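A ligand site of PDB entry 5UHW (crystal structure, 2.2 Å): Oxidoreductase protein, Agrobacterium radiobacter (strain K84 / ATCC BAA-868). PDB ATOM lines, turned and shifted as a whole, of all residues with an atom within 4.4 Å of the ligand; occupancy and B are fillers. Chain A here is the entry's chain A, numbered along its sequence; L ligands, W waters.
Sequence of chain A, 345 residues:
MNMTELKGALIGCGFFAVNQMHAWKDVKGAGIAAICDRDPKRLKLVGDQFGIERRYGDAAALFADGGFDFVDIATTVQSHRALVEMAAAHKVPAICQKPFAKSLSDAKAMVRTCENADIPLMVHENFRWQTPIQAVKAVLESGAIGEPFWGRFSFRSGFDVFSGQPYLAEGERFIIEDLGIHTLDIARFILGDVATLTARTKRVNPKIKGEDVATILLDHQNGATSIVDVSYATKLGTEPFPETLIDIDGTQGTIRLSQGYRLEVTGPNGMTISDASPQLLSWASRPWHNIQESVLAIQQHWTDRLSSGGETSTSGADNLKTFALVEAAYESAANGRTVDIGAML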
ATOM      1  N   ILE A  11       9.558  12.366   4.804  1.00  0.00           N
ATOM      2  CA  ILE A  11       8.320  12.465   5.534  1.00  0.00           C
ATOM      3  C   ILE A  11       7.564  11.143   5.362  1.00  0.00           C
ATOM      4  O   ILE A  11       7.131  10.813   4.259  1.00  0.00           O
ATOM      5  CB  ILE A  11       7.450  13.633   5.018  1.00  0.00           C
ATOM      6  CG1 ILE A  11       8.140  14.987   5.257  1.00  0.00           C
ATOM      7  CG2 ILE A  11       6.058  13.652   5.698  1.00  0.00           C
ATOM      8  CD1 ILE A  11       7.506  16.139   4.498  1.00  0.00           C
ATOM      9  N   GLY A  12       7.368  10.435   6.476  1.00  0.00           N
ATOM     10  CA  GLY A  12       6.718   9.117   6.515  1.00  0.00           C
ATOM     11  C   GLY A  12       7.724   8.005   6.723  1.00  0.00           C
ATOM     12  O   GLY A  12       8.196   7.382   5.755  1.00  0.00           O
ATOM     13  N   CYS A  13       8.049   7.730   8.001  1.00  0.00           N
ATOM     14  CA  CYS A  13       9.092   6.767   8.386  1.00  0.00           C
ATOM     15  C   CYS A  13       8.505   5.384   8.624  1.00  0.00           C
ATOM     16  O   CYS A  13       8.705   4.792   9.693  1.00  0.00           O
ATOM     17  CB  CYS A  13       9.781   7.227   9.665  1.00  0.00           C
ATOM     18  SG  CYS A  13      10.605   8.817   9.541  1.00  0.00           S
ATOM     19  N   GLY A  14       7.768   4.879   7.637  1.00  0.00           N
ATOM     20  CA  GLY A  14       7.114   3.585   7.754  1.00  0.00           C
ATOM     21  C   GLY A  14       7.957   2.466   7.204  1.00  0.00           C
ATOM     22  O   GLY A  14       9.183   2.584   7.105  1.00  0.00           O
ATOM     23  N   PHE A  15       7.295   1.366   6.837  1.00  0.00           N
ATOM     24  CA  PHE A  15       7.997   0.126   6.516  1.00  0.00           C
ATOM     25  C   PHE A  15       8.842   0.290   5.241  1.00  0.00           C
ATOM     26  O   PHE A  15      10.030  -0.031   5.263  1.00  0.00           O
ATOM     27  CB  PHE A  15       7.036  -1.106   6.506  1.00  0.00           C
ATOM     28  CG  PHE A  15       6.451  -1.454   7.891  1.00  0.00           C
ATOM     29  CD1 PHE A  15       7.236  -1.387   9.076  1.00  0.00           C
ATOM     30  CD2 PHE A  15       5.104  -1.870   8.025  1.00  0.00           C
ATOM     31  CE1 PHE A  15       6.690  -1.688  10.331  1.00  0.00           C
ATOM     32  CE2 PHE A  15       4.553  -2.179   9.280  1.00  0.00           C
ATOM     33  CZ  PHE A  15       5.351  -2.074  10.443  1.00  0.00           C
ATOM     34  N   PHE A  16       8.275   0.851   4.174  1.00  0.00           N
ATOM     35  CA  PHE A  16       9.073   1.038   2.971  1.00  0.00           C
ATOM     36  C   PHE A  16      10.126   2.168   3.055  1.00  0.00           C
ATOM     37  O   PHE A  16      11.181   2.082   2.415  1.00  0.00           O
ATOM     38  CB  PHE A  16       8.222   1.182   1.728  1.00  0.00           C
ATOM     39  CG  PHE A  16       8.966   0.838   0.446  1.00  0.00           C
ATOM     40  CD1 PHE A  16       9.195  -0.479   0.083  1.00  0.00           C
ATOM     41  CD2 PHE A  16       9.440   1.833  -0.390  1.00  0.00           C
ATOM     42  CE1 PHE A  16       9.863  -0.797  -1.101  1.00  0.00           C
ATOM     43  CE2 PHE A  16      10.105   1.527  -1.586  1.00  0.00           C
ATOM     44  CZ  PHE A  16      10.314   0.219  -1.942  1.00  0.00           C
ATOM     45  N   ALA A  17       9.891   3.198   3.857  1.00  0.00           N
ATOM     46  CA  ALA A  17      10.904   4.281   4.020  1.00  0.00           C
ATOM     47  C   ALA A  17      12.245   3.784   4.520  1.00  0.00           C
ATOM     48  O   ALA A  17      13.248   4.403   4.231  1.00  0.00           O
ATOM     49  CB  ALA A  17      10.393   5.358   4.946  1.00  0.00           C
ATOM     50  N   CYS A  36      10.398  13.070   9.424  1.00  0.00           N
ATOM     51  CA  CYS A  36       9.116  13.403   9.996  1.00  0.00           C
ATOM     52  C   CYS A  36       8.210  12.189   9.983  1.00  0.00           C
ATOM     53  O   CYS A  36       8.122  11.475   8.979  1.00  0.00           O
ATOM     54  CB  CYS A  36       8.464  14.519   9.185  1.00  0.00           C
ATOM     55  SG  CYS A  36       6.775  14.987   9.687  1.00  0.00           S
ATOM     56  N   ASP A  37       7.566  11.937  11.117  1.00  0.00           N
ATOM     57  CA  ASP A  37       6.473  10.983  11.204  1.00  0.00           C
ATOM     58  C   ASP A  37       5.523  11.373  12.335  1.00  0.00           C
ATOM     59  O   ASP A  37       5.911  11.816  13.433  1.00  0.00           O
ATOM     60  CB  ASP A  37       6.960   9.536  11.424  1.00  0.00           C
ATOM     61  CG  ASP A  37       5.918   8.480  10.969  1.00  0.00           C
ATOM     62  OD1 ASP A  37       4.800   8.385  11.532  1.00  0.00           O
ATOM     63  OD2 ASP A  37       6.227   7.726  10.035  1.00  0.00           O
ATOM     64  N   ARG A  38       4.251  11.156  12.038  1.00  0.00           N
ATOM     65  CA  ARG A  38       3.146  11.445  12.907  1.00  0.00           C
ATOM     66  C   ARG A  38       3.158  10.488  14.117  1.00  0.00           C
ATOM     67  O   ARG A  38       2.659  10.823  15.185  1.00  0.00           O
ATOM     68  CB  ARG A  38       1.890  11.253  12.051  1.00  0.00           C
ATOM     69  CG  ARG A  38       0.717  12.045  12.481  1.00  0.00           C
ATOM     70  CD  ARG A  38      -0.393  11.938  11.449  1.00  0.00           C
ATOM     71  NE  ARG A  38      -0.469  13.115  10.578  1.00  0.00           N
ATOM     72  CZ  ARG A  38      -1.573  13.562   9.969  1.00  0.00           C
ATOM     73  NH1 ARG A  38      -2.746  12.949  10.107  1.00  0.00           N
ATOM     74  NH2 ARG A  38      -1.514  14.650   9.219  1.00  0.00           N
ATOM     75  N   ASP A  39       3.779   9.311  13.950  1.00  0.00           N
ATOM     76  CA  ASP A  39       3.864   8.263  14.976  1.00  0.00           C
ATOM     77  C   ASP A  39       5.262   8.306  15.614  1.00  0.00           C
ATOM     78  O   ASP A  39       6.244   8.055  14.934  1.00  0.00           O
ATOM     79  CB  ASP A  39       3.554   6.911  14.281  1.00  0.00           C
ATOM     80  CG  ASP A  39       3.740   5.691  15.175  1.00  0.00           C
ATOM     81  OD1 ASP A  39       4.151   5.820  16.342  1.00  0.00           O
ATOM     82  OD2 ASP A  39       3.474   4.562  14.693  1.00  0.00           O
ATOM     83  N   ARG A  42       7.782   5.229  15.270  1.00  0.00           N
ATOM     84  CA  ARG A  42       8.470   5.136  13.979  1.00  0.00           C
ATOM     85  C   ARG A  42       9.550   6.197  13.830  1.00  0.00           C
ATOM     86  O   ARG A  42      10.654   5.930  13.345  1.00  0.00           O
ATOM     87  CB  ARG A  42       7.484   5.246  12.818  1.00  0.00           C
ATOM     88  CG  ARG A  42       6.451   4.118  12.696  1.00  0.00           C
ATOM     89  CD  ARG A  42       7.093   2.751  12.580  1.00  0.00           C
ATOM     90  NE  ARG A  42       8.010   2.701  11.435  1.00  0.00           N
ATOM     91  CZ  ARG A  42       8.802   1.684  11.153  1.00  0.00           C
ATOM     92  NH1 ARG A  42       8.847   0.612  11.929  1.00  0.00           N
ATOM     93  NH2 ARG A  42       9.555   1.737  10.064  1.00  0.00           N
ATOM     94  N   ALA A  74       7.100   9.560   1.700  1.00  0.00           N
ATOM     95  CA  ALA A  74       6.890   8.135   1.771  1.00  0.00           C
ATOM     96  C   ALA A  74       5.679   7.774   2.635  1.00  0.00           C
ATOM     97  O   ALA A  74       5.595   6.676   3.158  1.00  0.00           O
ATOM     98  CB  ALA A  74       8.152   7.476   2.322  1.00  0.00           C
ATOM     99  N   THR A  75       4.768   8.727   2.791  1.00  0.00           N
ATOM    100  CA  THR A  75       3.553   8.490   3.542  1.00  0.00           C
ATOM    101  C   THR A  75       2.592   7.717   2.661  1.00  0.00           C
ATOM    102  O   THR A  75       2.845   7.516   1.458  1.00  0.00           O
ATOM    103  CB  THR A  75       2.872   9.786   4.004  1.00  0.00           C
ATOM    104  OG1 THR A  75       2.490  10.580   2.878  1.00  0.00           O
ATOM    105  CG2 THR A  75       3.798  10.565   4.900  1.00  0.00           C
ATOM    106  N   THR A  76       1.517   7.256   3.291  1.00  0.00           N
ATOM    107  CA  THR A  76       0.380   6.659   2.590  1.00  0.00           C
ATOM    108  C   THR A  76      -0.346   7.756   1.819  1.00  0.00           C
ATOM    109  O   THR A  76      -0.150   8.942   2.060  1.00  0.00           O
ATOM    110  CB  THR A  76      -0.588   5.932   3.545  1.00  0.00           C
ATOM    111  OG1 THR A  76      -0.879   6.777   4.668  1.00  0.00           O
ATOM    112  CG2 THR A  76       0.043   4.693   4.057  1.00  0.00           C
ATOM    113  N   VAL A  77      -1.178   7.310   0.882  1.00  0.00           N
ATOM    114  CA  VAL A  77      -1.796   8.165  -0.116  1.00  0.00           C
ATOM    115  C   VAL A  77      -2.590   9.383   0.384  1.00  0.00           C
ATOM    116  O   VAL A  77      -2.471  10.429  -0.210  1.00  0.00           O
ATOM    117  CB  VAL A  77      -2.663   7.312  -1.087  1.00  0.00           C
ATOM    118  CG1 VAL A  77      -3.892   6.737  -0.371  1.00  0.00           C
ATOM    119  CG2 VAL A  77      -3.024   8.096  -2.341  1.00  0.00           C
ATOM    120  N   SER A  79      -2.219  11.673   2.579  1.00  0.00           N
ATOM    121  CA  SER A  79      -1.491  12.908   2.834  1.00  0.00           C
ATOM    122  C   SER A  79      -0.652  13.409   1.632  1.00  0.00           C
ATOM    123  O   SER A  79      -0.110  14.502   1.685  1.00  0.00           O
ATOM    124  CB  SER A  79      -0.638  12.729   4.091  1.00  0.00           C
ATOM    125  OG  SER A  79       0.336  11.722   3.889  1.00  0.00           O
ATOM    126  N   HIS A  80      -0.593  12.657   0.544  1.00  0.00           N
ATOM    127  CA  HIS A  80       0.290  13.024  -0.589  1.00  0.00           C
ATOM    128  C   HIS A  80       0.057  14.435  -1.130  1.00  0.00           C
ATOM    129  O   HIS A  80       1.023  15.207  -1.316  1.00  0.00           O
ATOM    130  CB  HIS A  80       0.187  12.050  -1.758  1.00  0.00           C
ATOM    131  CG  HIS A  80       0.813  10.725  -1.484  1.00  0.00           C
ATOM    132  ND1 HIS A  80       0.809   9.691  -2.397  1.00  0.00           N
ATOM    133  CD2 HIS A  80       1.435  10.248  -0.374  1.00  0.00           C
ATOM    134  CE1 HIS A  80       1.430   8.646  -1.872  1.00  0.00           C
ATOM    135  NE2 HIS A  80       1.803   8.950  -0.644  1.00  0.00           N
ATOM    136  N   GLN A  97       5.705   9.175  -3.151  1.00  0.00           N
ATOM    137  CA  GLN A  97       5.388   7.748  -3.332  1.00  0.00           C
ATOM    138  C   GLN A  97       4.114   7.510  -4.157  1.00  0.00           C
ATOM    139  O   GLN A  97       3.250   8.373  -4.281  1.00  0.00           O
ATOM    140  CB  GLN A  97       5.296   6.988  -1.973  1.00  0.00           C
ATOM    141  CG  GLN A  97       6.590   6.247  -1.553  1.00  0.00           C
ATOM    142  CD  GLN A  97       6.906   5.065  -2.452  1.00  0.00           C
ATOM    143  OE1 GLN A  97       6.109   4.736  -3.332  1.00  0.00           O
ATOM    144  NE2 GLN A  97       8.077   4.418  -2.253  1.00  0.00           N
ATOM    145  N   LYS A  98       4.024   6.306  -4.684  1.00  0.00           N
ATOM    146  CA  LYS A  98       2.806   5.850  -5.319  1.00  0.00           C
ATOM    147  C   LYS A  98       1.907   5.244  -4.241  1.00  0.00           C
ATOM    148  O   LYS A  98       2.381   4.963  -3.152  1.00  0.00           O
ATOM    149  CB  LYS A  98       3.074   4.859  -6.455  1.00  0.00           C
ATOM    150  CG  LYS A  98       4.085   3.734  -6.245  1.00  0.00           C
ATOM    151  CD  LYS A  98       3.825   2.812  -5.063  1.00  0.00           C
ATOM    152  CE  LYS A  98       2.522   2.040  -5.219  1.00  0.00           C
ATOM    153  NZ  LYS A  98       2.365   1.011  -4.134  1.00  0.00           N
ATOM    154  N   PRO A  99       0.610   5.072  -4.526  1.00  0.00           N
ATOM    155  CA  PRO A  99      -0.072   5.769  -5.643  1.00  0.00           C
ATOM    156  C   PRO A  99      -0.001   7.306  -5.492  1.00  0.00           C
ATOM    157  O   PRO A  99      -0.015   7.836  -4.378  1.00  0.00           O
ATOM    158  CB  PRO A  99      -1.524   5.260  -5.550  1.00  0.00           C
ATOM    159  CG  PRO A  99      -1.620   4.446  -4.300  1.00  0.00           C
ATOM    160  CD  PRO A  99      -0.335   4.545  -3.533  1.00  0.00           C
ATOM    161  N   HIS A 124       7.806   8.376  -6.965  1.00  0.00           N
ATOM    162  CA  HIS A 124       8.686   7.248  -6.675  1.00  0.00           C
ATOM    163  C   HIS A 124       8.016   5.996  -7.255  1.00  0.00           C
ATOM    164  O   HIS A 124       7.338   5.270  -6.546  1.00  0.00           O
ATOM    165  CB  HIS A 124       8.921   7.073  -5.166  1.00  0.00           C
ATOM    166  CG  HIS A 124      10.004   6.091  -4.854  1.00  0.00           C
ATOM    167  ND1 HIS A 124      11.182   6.455  -4.248  1.00  0.00           N
ATOM    168  CD2 HIS A 124      10.114   4.764  -5.103  1.00  0.00           C
ATOM    169  CE1 HIS A 124      11.963   5.398  -4.133  1.00  0.00           C
ATOM    170  NE2 HIS A 124      11.333   4.350  -4.641  1.00  0.00           N
ATOM    171  N   ASN A 126       9.229   2.764  -8.832  1.00  0.00           N
ATOM    172  CA  ASN A 126      10.506   2.110  -8.941  1.00  0.00           C
ATOM    173  C   ASN A 126      10.594   0.818  -9.767  1.00  0.00           C
ATOM    174  O   ASN A 126      11.692   0.398 -10.098  1.00  0.00           O
ATOM    175  CB  ASN A 126      11.189   1.960  -7.563  1.00  0.00           C
ATOM    176  CG  ASN A 126      10.385   1.151  -6.554  1.00  0.00           C
ATOM    177  OD1 ASN A 126       9.623   0.268  -6.904  1.00  0.00           O
ATOM    178  ND2 ASN A 126      10.607   1.452  -5.269  1.00  0.00           N
ATOM    179  N   PHE A 127       9.465   0.228 -10.163  1.00  0.00           N
ATOM    180  CA  PHE A 127       9.504  -1.040 -10.917  1.00  0.00           C
ATOM    181  C   PHE A 127      10.215  -0.932 -12.221  1.00  0.00           C
ATOM    182  O   PHE A 127      11.026  -1.779 -12.514  1.00  0.00           O
ATOM    183  CB  PHE A 127       8.131  -1.687 -11.095  1.00  0.00           C
ATOM    184  CG  PHE A 127       7.717  -2.566  -9.943  1.00  0.00           C
ATOM    185  CD1 PHE A 127       7.734  -2.075  -8.638  1.00  0.00           C
ATOM    186  CD2 PHE A 127       7.261  -3.869 -10.147  1.00  0.00           C
ATOM    187  CE1 PHE A 127       7.339  -2.874  -7.550  1.00  0.00           C
ATOM    188  CE2 PHE A 127       6.854  -4.674  -9.072  1.00  0.00           C
ATOM    189  CZ  PHE A 127       6.882  -4.165  -7.776  1.00  0.00           C
ATOM    190  N   GLN A 165       2.464  -5.770   5.702  1.00  0.00           N
ATOM    191  CA  GLN A 165       1.608  -4.577   5.726  1.00  0.00           C
ATOM    192  C   GLN A 165       0.080  -4.880   5.800  1.00  0.00           C
ATOM    193  O   GLN A 165      -0.565  -5.039   4.758  1.00  0.00           O
ATOM    194  CB  GLN A 165       1.944  -3.703   4.501  1.00  0.00           C
ATOM    195  CG  GLN A 165       1.370  -2.292   4.564  1.00  0.00           C
ATOM    196  CD  GLN A 165       1.660  -1.567   5.876  1.00  0.00           C
ATOM    197  OE1 GLN A 165       0.851  -1.592   6.810  1.00  0.00           O
ATOM    198  NE2 GLN A 165       2.829  -0.930   5.979  1.00  0.00           N
ATOM    199  N   TYR A 167      -2.800  -3.188   6.430  1.00  0.00           N
ATOM    200  CA  TYR A 167      -3.838  -2.293   5.857  1.00  0.00           C
ATOM    201  C   TYR A 167      -4.327  -2.785   4.472  1.00  0.00           C
ATOM    202  O   TYR A 167      -5.486  -2.568   4.118  1.00  0.00           O
ATOM    203  CB  TYR A 167      -3.426  -0.779   5.843  1.00  0.00           C
ATOM    204  CG  TYR A 167      -2.372  -0.295   4.821  1.00  0.00           C
ATOM    205  CD1 TYR A 167      -2.612  -0.285   3.437  1.00  0.00           C
ATOM    206  CD2 TYR A 167      -1.127   0.226   5.262  1.00  0.00           C
ATOM    207  CE1 TYR A 167      -1.657   0.158   2.524  1.00  0.00           C
ATOM    208  CE2 TYR A 167      -0.158   0.697   4.349  1.00  0.00           C
ATOM    209  CZ  TYR A 167      -0.427   0.653   2.974  1.00  0.00           C
ATOM    210  OH  TYR A 167       0.510   1.083   2.059  1.00  0.00           O
ATOM    211  N   HIS A 182       2.174  -0.524 -10.745  1.00  0.00           N
ATOM    212  CA  HIS A 182       3.525  -0.779 -11.240  1.00  0.00           C
ATOM    213  C   HIS A 182       3.571  -1.458 -12.642  1.00  0.00           C
ATOM    214  O   HIS A 182       4.375  -1.074 -13.515  1.00  0.00           O
ATOM    215  CB  HIS A 182       4.298  -1.677 -10.274  1.00  0.00           C
ATOM    216  CG  HIS A 182       4.533  -1.070  -8.921  1.00  0.00           C
ATOM    217  ND1 HIS A 182       5.158   0.149  -8.753  1.00  0.00           N
ATOM    218  CD2 HIS A 182       4.277  -1.548  -7.684  1.00  0.00           C
ATOM    219  CE1 HIS A 182       5.271   0.392  -7.462  1.00  0.00           C
ATOM    220  NE2 HIS A 182       4.743  -0.619  -6.786  1.00  0.00           N
ATOM    221  N   ILE A 291      13.683  -4.991  -5.876  1.00  0.00           N
ATOM    222  CA  ILE A 291      12.956  -3.772  -5.589  1.00  0.00           C
ATOM    223  C   ILE A 291      13.898  -2.778  -4.860  1.00  0.00           C
ATOM    224  O   ILE A 291      13.925  -1.563  -5.148  1.00  0.00           O
ATOM    225  CB  ILE A 291      11.673  -4.120  -4.779  1.00  0.00           C
ATOM    226  CG1 ILE A 291      10.650  -4.806  -5.698  1.00  0.00           C
ATOM    227  CG2 ILE A 291      11.077  -2.900  -4.083  1.00  0.00           C
ATOM    228  CD1 ILE A 291       9.465  -5.370  -4.945  1.00  0.00           C
HETATM  229  P1  LIG L   1       3.368   2.541   6.357  1.00  0.00           P
HETATM  230  O1  LIG L   1       1.965   2.665   6.904  1.00  0.00           O
HETATM  231  O2  LIG L   1       4.308   1.472   6.825  1.00  0.00           O
HETATM  232  O3  LIG L   1       4.125   3.940   6.542  1.00  0.00           O
HETATM  233  C1  LIG L   1       3.502   5.219   6.415  1.00  0.00           C
HETATM  234  C2  LIG L   1       4.059   6.080   7.537  1.00  0.00           C
HETATM  235  O4  LIG L   1       3.669   7.434   7.341  1.00  0.00           O
HETATM  236  C3  LIG L   1       3.539   5.654   8.908  1.00  0.00           C
HETATM  237  O5  LIG L   1       4.659   5.489   9.791  1.00  0.00           O
HETATM  238  C4  LIG L   1       2.626   6.775   9.366  1.00  0.00           C
HETATM  239  O6  LIG L   1       2.699   7.005  10.763  1.00  0.00           O
HETATM  240  C5  LIG L   1       3.171   7.957   8.578  1.00  0.00           C
HETATM  241  N1  LIG L   1       2.254   9.037   8.193  1.00  0.00           N
HETATM  242  C6  LIG L   1       1.032   8.929   7.641  1.00  0.00           C
HETATM  243  N2  LIG L   1       0.546  10.174   7.377  1.00  0.00           N
HETATM  244  C7  LIG L   1       1.475  11.086   7.753  1.00  0.00           C
HETATM  245  C8  LIG L   1       1.616  12.567   7.768  1.00  0.00           C
HETATM  246  N3  LIG L   1       0.624  13.371   7.302  1.00  0.00           N
HETATM  247  N4  LIG L   1       2.779  13.073   8.237  1.00  0.00           N
HETATM  248  C9  LIG L   1       3.783  12.296   8.713  1.00  0.00           C
HETATM  249  N5  LIG L   1       3.715  10.957   8.740  1.00  0.00           N
HETATM  250  C10 LIG L   1       2.615  10.309   8.282  1.00  0.00           C
HETATM  251  O7  LIG L   1       3.211   2.465   4.749  1.00  0.00           O
HETATM  252  P2  LIG L   1       4.301   1.759   3.779  1.00  0.00           P
HETATM  253  O8  LIG L   1       4.001   0.290   3.686  1.00  0.00           O
HETATM  254  O9  LIG L   1       5.684   2.234   4.156  1.00  0.00           O
HETATM  255  O10 LIG L   1       3.902   2.450   2.374  1.00  0.00           O
HETATM  256  C11 LIG L   1       4.029   3.849   2.261  1.00  0.00           C
HETATM  257  C12 LIG L   1       3.809   4.239   0.809  1.00  0.00           C
HETATM  258  O11 LIG L   1       4.822   3.616   0.023  1.00  0.00           O
HETATM  259  C13 LIG L   1       2.458   3.793   0.293  1.00  0.00           C
HETATM  260  O12 LIG L   1       1.870   4.855  -0.462  1.00  0.00           O
HETATM  261  C14 LIG L   1       2.754   2.599  -0.587  1.00  0.00           C
HETATM  262  O13 LIG L   1       1.898   2.544  -1.733  1.00  0.00           O
HETATM  263  C15 LIG L   1       4.215   2.835  -0.992  1.00  0.00           C
HETATM  264  N6  LIG L   1       5.021   1.622  -1.205  1.00  0.00           N
HETATM  265  C16 LIG L   1       5.794   1.598  -2.305  1.00  0.00           C
HETATM  266  C17 LIG L   1       6.593   0.511  -2.621  1.00  0.00           C
HETATM  267  C18 LIG L   1       7.466   0.561  -3.862  1.00  0.00           C
HETATM  268  O14 LIG L   1       7.937   1.634  -4.227  1.00  0.00           O
HETATM  269  N7  LIG L   1       7.751  -0.550  -4.548  1.00  0.00           N
HETATM  270  C19 LIG L   1       6.573  -0.585  -1.752  1.00  0.00           C
HETATM  271  C20 LIG L   1       5.771  -0.558  -0.617  1.00  0.00           C
HETATM  272  C21 LIG L   1       4.992   0.575  -0.342  1.00  0.00           C
HETATM  273  O   HOH W   1      -1.079   4.507   0.170  1.00  0.00           O
HETATM  274  O   HOH W   2       4.250  -1.507  -3.969  1.00  0.00           O
HETATM  275  O   HOH W   3       7.208   4.480   4.686  1.00  0.00           O
HETATM  276  O   HOH W   4       7.429   2.603  -6.568  1.00  0.00           O
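The backbone NH (N) of Asp 39 lies within hydrogen-bond range of the side-chain carboxylate (OD1) of Asp 37 (2.8 Å). The side-chain carboxylate of Asp 37 lies within hydrogen-bond range of the backbone NH of Cys 13, 2.7 Å away. The backbone carbonyl oxygen (O) of Gly 14 sits at hydrogen-bond distance from the guanidinium group (NH2) of Arg 42, 3.1 Å away. The side-chain amide oxygen of Gln 97 lies close to the backbone carbonyl oxygen of His 124, at 3.5 Å. The side-chain hydroxyl (OG1) of Thr 75 is in hydrogen-bond range of the side-chain hydroxyl (OG) of Ser 79, 2.6 Å away. The backbone NH (N) of Thr 75 lies close to the backbone carbonyl oxygen (O) of Ile 11 (3.5 Å). NE2 of His 80 sits at hydrogen-bond distance from O of Thr 75 (2.7 Å). OG of Ser 79 lies within hydrogen-bond range of O of Thr 76, 3.4 Å away.
An oxygen (O6) of the ligand lies within hydrogen-bond range of the side-chain carboxylate (OD1) of Asp 37. An oxygen (O12) of the ligand sits at hydrogen-bond distance from the backbone carbonyl oxygen of Lys 98, 2.7 Å away. The side-chain amino group (NZ) of Lys 98 lies within hydrogen-bond range of an oxygen (O13) of the ligand, at 2.9 Å. An oxygen (O8) of the ligand sits at hydrogen-bond distance from the side-chain amide nitrogen (NE2) of Gln 165 (2.8 Å). ND2 of Asn 126 lies within hydrogen-bond range of O14 of the ligand. N of Phe 16 is in hydrogen-bond range of O9 of the ligand. The backbone NH of Phe 15 is in hydrogen-bond range of an oxygen (O2) of the ligand (3.0 Å). The backbone NH (N) of Arg 38 lies within hydrogen-bond range of a nitrogen (N5) of the ligand. An oxygen (O14) of the ligand is in hydrogen-bond range of the side-chain amide nitrogen (NE2) of Gln 97, 3.4 Å away. The backbone carbonyl oxygen of Thr 75 lies within hydrogen-bond range of an oxygen (O12) of the ligand (3.4 Å).
CA of Gly 12 touches O4 of the ligand (3.6 Å). Gly 14 touches the ligand. Asp 39 touches the ligand. Arg 42 touches the ligand (CG to O5, 3.7 Å). O of Ala 74 touches C11 of the ligand, at 3.4 Å. Thr 76 touches the ligand (CA to O12, 3.8 Å). Ser 79 touches the ligand. Pro 99 touches the ligand. His 124 touches the ligand (CD2 to O14, 3.9 Å). Phe 127 touches the ligand. Tyr 167 touches the ligand (OH to O10, 3.7 Å). His 182 touches the ligand (NE2 to N7, 3.7 Å). Within 4 Å of the ligand: Gly 12, Gly 14, Phe 15, Phe 16, Asp 37, Arg 38, Asp 39, Arg 42, Ala 74, Thr 75, Thr 76, Ser 79, Gln 97, Lys 98, Pro 99, His 124, Asn 126, Phe 127, Gln 165, Tyr 167 and His 182. The nearest printed residue that does not touch the ligand is Ile 11 (4.01 Å).
Water W4 lies within hydrogen-bond range of O14 of the ligand (2.6 Å), O of His 124 (2.7 Å) and N of Asn 126 (2.9 Å). Water W3 lies within hydrogen-bond range of O9 of the ligand (2.8 Å), N of Gly 14 (3.0 Å), N of Ala 17 (3.1 Å), O of Ala 74 (3.1 Å) and O of Gly 12 (3.2 Å). Water W1 bridges N of Val 77 (2.9 Å) and O12 of the ligand (3.0 Å). Water W2 bridges a ring nitrogen (NE2) of His 182 (3.0 Å) and the side-chain amino group (NZ) of Lys 98 (3.1 Å).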
